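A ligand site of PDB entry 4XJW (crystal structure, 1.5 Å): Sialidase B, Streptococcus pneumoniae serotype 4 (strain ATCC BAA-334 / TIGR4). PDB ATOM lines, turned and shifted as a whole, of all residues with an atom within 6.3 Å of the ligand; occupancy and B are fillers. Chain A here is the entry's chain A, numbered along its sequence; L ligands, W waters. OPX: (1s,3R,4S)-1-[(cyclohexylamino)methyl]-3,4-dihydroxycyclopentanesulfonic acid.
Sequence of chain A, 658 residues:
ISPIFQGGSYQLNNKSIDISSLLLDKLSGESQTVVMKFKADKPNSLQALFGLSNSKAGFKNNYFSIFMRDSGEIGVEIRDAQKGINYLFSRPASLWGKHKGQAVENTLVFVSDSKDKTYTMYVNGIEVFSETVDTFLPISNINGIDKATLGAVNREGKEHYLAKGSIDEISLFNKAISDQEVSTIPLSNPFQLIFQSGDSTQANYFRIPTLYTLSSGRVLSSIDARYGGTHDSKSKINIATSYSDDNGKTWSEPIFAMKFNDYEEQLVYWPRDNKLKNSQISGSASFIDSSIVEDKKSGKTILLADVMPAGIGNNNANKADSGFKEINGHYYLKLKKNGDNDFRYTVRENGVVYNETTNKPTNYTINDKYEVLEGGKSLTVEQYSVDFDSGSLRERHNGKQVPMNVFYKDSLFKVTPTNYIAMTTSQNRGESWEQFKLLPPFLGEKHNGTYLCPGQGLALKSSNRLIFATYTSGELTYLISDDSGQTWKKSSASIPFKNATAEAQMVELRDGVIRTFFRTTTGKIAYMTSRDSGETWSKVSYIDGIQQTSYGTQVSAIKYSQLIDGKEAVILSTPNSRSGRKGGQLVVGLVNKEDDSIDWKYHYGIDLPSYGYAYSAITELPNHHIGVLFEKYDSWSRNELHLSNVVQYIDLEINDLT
Tyr 212 touches the ligand. Lys 461 touches the ligand (CE to OAA, 3.5 Å). Ile 558 touches the ligand. Glu 620 touches the ligand. Leu 621 touches the ligand (O to CAH, 3.6 Å). Pro 622 touches the ligand (CA to CAH, 3.98 Å). Hydrophobic or aromatic side chains that line the ligand: Tyr 212 and Ile 558.
O of Ile 618 lies within hydrogen-bond range of NE2 of Gln 456 (3.3 Å). The side-chain carboxylate (OE2) of Glu 620 is in hydrogen-bond range of a ring nitrogen (ND1) of His 624 (2.7 Å). NE2 of Gln 456 is in hydrogen-bond range of O of Leu 211 (2.8 Å). The side-chain hydroxyl of Thr 619 lies within hydrogen-bond range of the side-chain hydroxyl of Thr 213. O of Glu 620 sits at hydrogen-bond distance from OG1 of Thr 213, at 2.7 Å. The side-chain hydroxyl of Ser 561 lies within hydrogen-bond range of the side-chain carboxylate of Glu 620 (2.6 Å).
An oxygen (OAD) of the ligand sits at hydrogen-bond distance from the backbone NH of Thr 213 (3.0 Å). The side-chain amide oxygen (OE1) of Gln 456 is in hydrogen-bond range of an oxygen (OAC) of the ligand (2.8 Å). An oxygen (OAD) of the ligand sits at hydrogen-bond distance from the side-chain hydroxyl (OG1) of Thr 619.
Water W5 bridges an oxygen (OAE) of the ligand (2.6 Å) and the side-chain hydroxyl of Tyr 212 (2.7 Å). Water W2 lies within hydrogen-bond range of OH of Tyr 212 (2.7 Å), OAB of the ligand (2.7 Å) and N of Ala 459 (3.0 Å). Water W4 lies within hydrogen-bond range of OAC of the ligand, N of Glu 620 and OG1 of Thr 619. Water W1 bridges N of Lys 559 (2.9 Å) and OAC of the ligand (3.2 Å). Water W6 lies within hydrogen-bond range of OAA of the ligand (3.2 Å) and O of Lys 559 (3.2 Å). Water W3 bridges O of Thr 213 and OAE of the ligand.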
ATOM      1  N   LEU A 211      19.941  31.619  30.657  1.00  0.00           N
ATOM      2  CA  LEU A 211      18.504  31.396  30.859  1.00  0.00           C
ATOM      3  C   LEU A 211      18.155  30.018  30.333  1.00  0.00           C
ATOM      4  O   LEU A 211      18.739  29.563  29.358  1.00  0.00           O
ATOM      5  CB  LEU A 211      17.692  32.433  30.072  1.00  0.00           C
ATOM      6  CG  LEU A 211      17.638  33.883  30.528  1.00  0.00           C
ATOM      7  CD1 LEU A 211      16.953  34.757  29.477  1.00  0.00           C
ATOM      8  CD2 LEU A 211      16.955  33.997  31.879  1.00  0.00           C
ATOM      9  N   TYR A 212      17.194  29.349  30.962  1.00  0.00           N
ATOM     10  CA  TYR A 212      16.770  28.034  30.523  1.00  0.00           C
ATOM     11  C   TYR A 212      15.355  27.812  31.000  1.00  0.00           C
ATOM     12  O   TYR A 212      15.027  28.085  32.164  1.00  0.00           O
ATOM     13  CB  TYR A 212      17.683  26.963  31.120  1.00  0.00           C
ATOM     14  CG  TYR A 212      17.560  25.586  30.492  1.00  0.00           C
ATOM     15  CD1 TYR A 212      16.508  24.740  30.823  1.00  0.00           C
ATOM     16  CD2 TYR A 212      18.499  25.142  29.590  1.00  0.00           C
ATOM     17  CE1 TYR A 212      16.407  23.474  30.254  1.00  0.00           C
ATOM     18  CE2 TYR A 212      18.414  23.892  29.019  1.00  0.00           C
ATOM     19  CZ  TYR A 212      17.373  23.054  29.360  1.00  0.00           C
ATOM     20  OH  TYR A 212      17.300  21.815  28.774  1.00  0.00           O
ATOM     21  N   THR A 213      14.505  27.306  30.112  1.00  0.00           N
ATOM     22  CA  THR A 213      13.100  27.085  30.446  1.00  0.00           C
ATOM     23  C   THR A 213      12.903  25.619  30.829  1.00  0.00           C
ATOM     24  O   THR A 213      13.113  24.728  30.007  1.00  0.00           O
ATOM     25  CB  THR A 213      12.198  27.451  29.282  1.00  0.00           C
ATOM     26  OG1 THR A 213      12.430  28.822  28.936  1.00  0.00           O
ATOM     27  CG2 THR A 213      10.726  27.264  29.635  1.00  0.00           C
ATOM     28  N   LEU A 214      12.514  25.407  32.081  1.00  0.00           N
ATOM     29  CA  LEU A 214      12.308  24.050  32.618  1.00  0.00           C
ATOM     30  C   LEU A 214      10.949  23.496  32.200  1.00  0.00           C
ATOM     31  O   LEU A 214      10.046  24.244  31.782  1.00  0.00           O
ATOM     32  CB  LEU A 214      12.443  24.053  34.143  1.00  0.00           C
ATOM     33  CG  LEU A 214      13.766  24.631  34.669  1.00  0.00           C
ATOM     34  CD1 LEU A 214      13.757  24.622  36.202  1.00  0.00           C
ATOM     35  CD2 LEU A 214      14.941  23.810  34.146  1.00  0.00           C
ATOM     36  N   GLN A 456      23.391  27.533  27.697  1.00  0.00           N
ATOM     37  CA  GLN A 456      22.589  26.324  27.814  1.00  0.00           C
ATOM     38  C   GLN A 456      23.375  25.112  27.399  1.00  0.00           C
ATOM     39  O   GLN A 456      24.172  25.151  26.458  1.00  0.00           O
ATOM     40  CB  GLN A 456      21.331  26.426  26.918  1.00  0.00           C
ATOM     41  CG  GLN A 456      20.388  27.592  27.272  1.00  0.00           C
ATOM     42  CD  GLN A 456      19.125  27.644  26.421  1.00  0.00           C
ATOM     43  OE1 GLN A 456      19.001  26.935  25.421  1.00  0.00           O
ATOM     44  NE2 GLN A 456      18.185  28.497  26.811  1.00  0.00           N
ATOM     45  N   GLY A 457      23.163  24.014  28.116  1.00  0.00           N
ATOM     46  CA  GLY A 457      23.476  22.699  27.584  1.00  0.00           C
ATOM     47  C   GLY A 457      22.274  22.289  26.743  1.00  0.00           C
ATOM     48  O   GLY A 457      21.267  23.032  26.687  1.00  0.00           O
ATOM     49  N   LEU A 458      22.357  21.125  26.106  1.00  0.00           N
ATOM     50  CA  LEU A 458      21.292  20.671  25.211  1.00  0.00           C
ATOM     51  C   LEU A 458      20.762  19.317  25.623  1.00  0.00           C
ATOM     52  O   LEU A 458      21.513  18.350  25.751  1.00  0.00           O
ATOM     53  CB  LEU A 458      21.820  20.592  23.782  1.00  0.00           C
ATOM     54  CG  LEU A 458      20.811  20.091  22.743  1.00  0.00           C
ATOM     55  CD1 LEU A 458      19.735  21.119  22.467  1.00  0.00           C
ATOM     56  CD2 LEU A 458      21.539  19.752  21.454  1.00  0.00           C
ATOM     57  N   ALA A 459      19.463  19.274  25.869  1.00  0.00           N
ATOM     58  CA  ALA A 459      18.758  18.030  26.124  1.00  0.00           C
ATOM     59  C   ALA A 459      18.066  17.634  24.835  1.00  0.00           C
ATOM     60  O   ALA A 459      17.286  18.388  24.268  1.00  0.00           O
ATOM     61  CB  ALA A 459      17.739  18.215  27.225  1.00  0.00           C
ATOM     62  N   LYS A 461      15.533  15.915  22.160  1.00  0.00           N
ATOM     63  CA  LYS A 461      14.081  15.712  22.180  1.00  0.00           C
ATOM     64  C   LYS A 461      13.647  14.246  22.308  1.00  0.00           C
ATOM     65  O   LYS A 461      12.698  13.949  23.029  1.00  0.00           O
ATOM     66  CB  LYS A 461      13.452  16.334  20.934  1.00  0.00           C
ATOM     67  CG  LYS A 461      13.466  17.855  20.901  1.00  0.00           C
ATOM     68  CD  LYS A 461      12.202  18.430  21.535  1.00  0.00           C
ATOM     69  CE  LYS A 461      12.251  19.957  21.647  1.00  0.00           C
ATOM     70  NZ  LYS A 461      12.338  20.638  20.322  1.00  0.00           N
ATOM     71  N   ALA A 557      21.557  31.019  21.248  1.00  0.00           N
ATOM     72  CA  ALA A 557      20.787  30.468  20.140  1.00  0.00           C
ATOM     73  C   ALA A 557      19.705  29.556  20.636  1.00  0.00           C
ATOM     74  O   ALA A 557      19.967  28.734  21.519  1.00  0.00           O
ATOM     75  CB  ALA A 557      21.705  29.717  19.192  1.00  0.00           C
ATOM     76  N   ILE A 558      18.518  29.675  20.067  1.00  0.00           N
ATOM     77  CA  ILE A 558      17.437  28.738  20.402  1.00  0.00           C
ATOM     78  C   ILE A 558      16.655  28.305  19.165  1.00  0.00           C
ATOM     79  O   ILE A 558      16.643  28.991  18.142  1.00  0.00           O
ATOM     80  CB  ILE A 558      16.433  29.335  21.423  1.00  0.00           C
ATOM     81  CG1 ILE A 558      15.784  30.614  20.867  1.00  0.00           C
ATOM     82  CG2 ILE A 558      17.114  29.611  22.754  1.00  0.00           C
ATOM     83  CD1 ILE A 558      14.553  31.083  21.659  1.00  0.00           C
ATOM     84  N   LYS A 559      16.006  27.150  19.286  1.00  0.00           N
ATOM     85  CA  LYS A 559      15.038  26.686  18.301  1.00  0.00           C
ATOM     86  C   LYS A 559      13.667  27.054  18.847  1.00  0.00           C
ATOM     87  O   LYS A 559      13.290  26.604  19.925  1.00  0.00           O
ATOM     88  CB  LYS A 559      15.163  25.167  18.136  1.00  0.00           C
ATOM     89  CG  LYS A 559      14.071  24.513  17.295  1.00  0.00           C
ATOM     90  CD  LYS A 559      14.323  24.716  15.822  1.00  0.00           C
ATOM     91  CE  LYS A 559      13.157  24.191  14.971  1.00  0.00           C
ATOM     92  NZ  LYS A 559      12.853  22.744  15.178  1.00  0.00           N
ATOM     93  N   SER A 561       9.650  27.127  19.270  1.00  0.00           N
ATOM     94  CA  SER A 561       8.688  26.020  19.230  1.00  0.00           C
ATOM     95  C   SER A 561       7.585  26.152  18.176  1.00  0.00           C
ATOM     96  O   SER A 561       6.959  25.165  17.804  1.00  0.00           O
ATOM     97  CB  SER A 561       8.034  25.817  20.613  1.00  0.00           C
ATOM     98  OG  SER A 561       7.051  26.804  20.876  1.00  0.00           O
ATOM     99  N   ILE A 618      19.233  33.824  25.787  1.00  0.00           N
ATOM    100  CA  ILE A 618      17.864  33.854  25.304  1.00  0.00           C
ATOM    101  C   ILE A 618      17.110  32.554  25.578  1.00  0.00           C
ATOM    102  O   ILE A 618      17.682  31.459  25.535  1.00  0.00           O
ATOM    103  CB  ILE A 618      17.763  34.218  23.807  1.00  0.00           C
ATOM    104  CG1 ILE A 618      18.565  33.247  22.935  1.00  0.00           C
ATOM    105  CG2 ILE A 618      18.201  35.684  23.576  1.00  0.00           C
ATOM    106  CD1 ILE A 618      18.317  33.472  21.442  1.00  0.00           C
ATOM    107  N   THR A 619      15.831  32.680  25.885  1.00  0.00           N
ATOM    108  CA  THR A 619      15.016  31.483  26.016  1.00  0.00           C
ATOM    109  C   THR A 619      13.589  31.776  25.647  1.00  0.00           C
ATOM    110  O   THR A 619      13.104  32.889  25.833  1.00  0.00           O
ATOM    111  CB  THR A 619      15.158  30.834  27.413  1.00  0.00           C
ATOM    112  OG1 THR A 619      14.783  29.455  27.330  1.00  0.00           O
ATOM    113  CG2 THR A 619      14.297  31.549  28.485  1.00  0.00           C
ATOM    114  N   GLU A 620      12.919  30.767  25.092  1.00  0.00           N
ATOM    115  CA  GLU A 620      11.488  30.861  24.865  1.00  0.00           C
ATOM    116  C   GLU A 620      10.789  30.616  26.182  1.00  0.00           C
ATOM    117  O   GLU A 620      10.980  29.567  26.821  1.00  0.00           O
ATOM    118  CB  GLU A 620      11.030  29.837  23.821  1.00  0.00           C
ATOM    119  CG  GLU A 620       9.538  29.932  23.506  1.00  0.00           C
ATOM    120  CD  GLU A 620       9.106  28.971  22.423  1.00  0.00           C
ATOM    121  OE1 GLU A 620       9.960  28.237  21.874  1.00  0.00           O
ATOM    122  OE2 GLU A 620       7.876  28.930  22.138  1.00  0.00           O
ATOM    123  N   LEU A 621      10.014  31.603  26.605  1.00  0.00           N
ATOM    124  CA  LEU A 621       9.207  31.493  27.810  1.00  0.00           C
ATOM    125  C   LEU A 621       8.036  30.551  27.506  1.00  0.00           C
ATOM    126  O   LEU A 621       7.676  30.352  26.324  1.00  0.00           O
ATOM    127  CB  LEU A 621       8.734  32.872  28.255  1.00  0.00           C
ATOM    128  CG  LEU A 621       9.908  33.855  28.386  1.00  0.00           C
ATOM    129  CD1 LEU A 621       9.442  35.274  28.556  1.00  0.00           C
ATOM    130  CD2 LEU A 621      10.841  33.450  29.526  1.00  0.00           C
ATOM    131  N   PRO A 622       7.452  29.950  28.546  1.00  0.00           N
ATOM    132  CA  PRO A 622       6.367  29.004  28.301  1.00  0.00           C
ATOM    133  C   PRO A 622       5.173  29.619  27.578  1.00  0.00           C
ATOM    134  O   PRO A 622       4.409  28.878  26.948  1.00  0.00           O
ATOM    135  CB  PRO A 622       5.943  28.570  29.704  1.00  0.00           C
ATOM    136  CG  PRO A 622       7.188  28.741  30.527  1.00  0.00           C
ATOM    137  CD  PRO A 622       7.851  29.974  29.967  1.00  0.00           C
ATOM    138  N   ASN A 623       5.006  30.929  27.641  1.00  0.00           N
ATOM    139  CA  ASN A 623       3.928  31.601  26.921  1.00  0.00           C
ATOM    140  C   ASN A 623       4.280  31.988  25.491  1.00  0.00           C
ATOM    141  O   ASN A 623       3.551  32.732  24.838  1.00  0.00           O
ATOM    142  CB  ASN A 623       3.453  32.833  27.704  1.00  0.00           C
ATOM    143  CG  ASN A 623       4.538  33.870  27.851  1.00  0.00           C
ATOM    144  OD1 ASN A 623       5.636  33.712  27.328  1.00  0.00           O
ATOM    145  ND2 ASN A 623       4.241  34.946  28.583  1.00  0.00           N
ATOM    146  N   HIS A 624       5.446  31.512  25.038  1.00  0.00           N
ATOM    147  CA  HIS A 624       5.963  31.737  23.687  1.00  0.00           C
ATOM    148  C   HIS A 624       6.515  33.136  23.431  1.00  0.00           C
ATOM    149  O   HIS A 624       6.853  33.467  22.300  1.00  0.00           O
ATOM    150  CB  HIS A 624       4.944  31.343  22.601  1.00  0.00           C
ATOM    151  CG  HIS A 624       4.421  29.954  22.768  1.00  0.00           C
ATOM    152  ND1 HIS A 624       5.243  28.845  22.802  1.00  0.00           N
ATOM    153  CD2 HIS A 624       3.157  29.482  22.917  1.00  0.00           C
ATOM    154  CE1 HIS A 624       4.513  27.754  22.964  1.00  0.00           C
ATOM    155  NE2 HIS A 624       3.247  28.115  23.028  1.00  0.00           N
HETATM  156  CAF OPX L   1       7.854  26.474  25.142  1.00  0.00           C
HETATM  157  CAG OPX L   1       7.791  24.978  25.115  1.00  0.00           C
HETATM  158  CAH OPX L   1       8.930  26.935  26.071  1.00  0.00           C
HETATM  159  CAI OPX L   1       9.116  24.390  24.753  1.00  0.00           C
HETATM  160  CAJ OPX L   1      10.266  26.354  25.742  1.00  0.00           C
HETATM  161  CAK OPX L   1      12.514  24.395  26.240  1.00  0.00           C
HETATM  162  CAL OPX L   1      14.557  25.059  24.853  1.00  0.00           C
HETATM  163  CAM OPX L   1      14.898  24.255  27.088  1.00  0.00           C
HETATM  164  CAO OPX L   1      15.879  25.503  25.370  1.00  0.00           C
HETATM  165  CAP OPX L   1      15.722  25.516  26.829  1.00  0.00           C
HETATM  166  CAQ OPX L   1      10.199  24.839  25.685  1.00  0.00           C
HETATM  167  CAR OPX L   1      13.997  24.102  25.872  1.00  0.00           C
HETATM  168  NAN OPX L   1      11.465  24.270  25.204  1.00  0.00           N
HETATM  169  OAA OPX L   1      13.218  22.340  24.050  1.00  0.00           O
HETATM  170  OAB OPX L   1      15.525  22.210  24.812  1.00  0.00           O
HETATM  171  OAC OPX L   1      16.234  26.744  24.866  1.00  0.00           O
HETATM  172  OAD OPX L   1      15.019  26.599  27.274  1.00  0.00           O
HETATM  173  OAE OPX L   1      13.759  21.494  26.270  1.00  0.00           O
HETATM  174  SAS OPX L   1      14.130  22.445  25.214  1.00  0.00           S
HETATM  175  O   HOH W   1      16.360  25.862  21.841  1.00  0.00           O
HETATM  176  O   HOH W   2      17.864  21.751  26.162  1.00  0.00           O
HETATM  177  O   HOH W   3      12.541  22.067  29.471  1.00  0.00           O
HETATM  178  O   HOH W   4      14.114  28.336  24.115  1.00  0.00           O
HETATM  179  O   HOH W   5      14.817  20.716  28.562  1.00  0.00           O
HETATM  180  O   HOH W   6      13.937  23.734  21.279  1.00  0.00           O
HETATM  181  O   HOH W   7      10.906  21.361  25.354  1.00  0.00           O
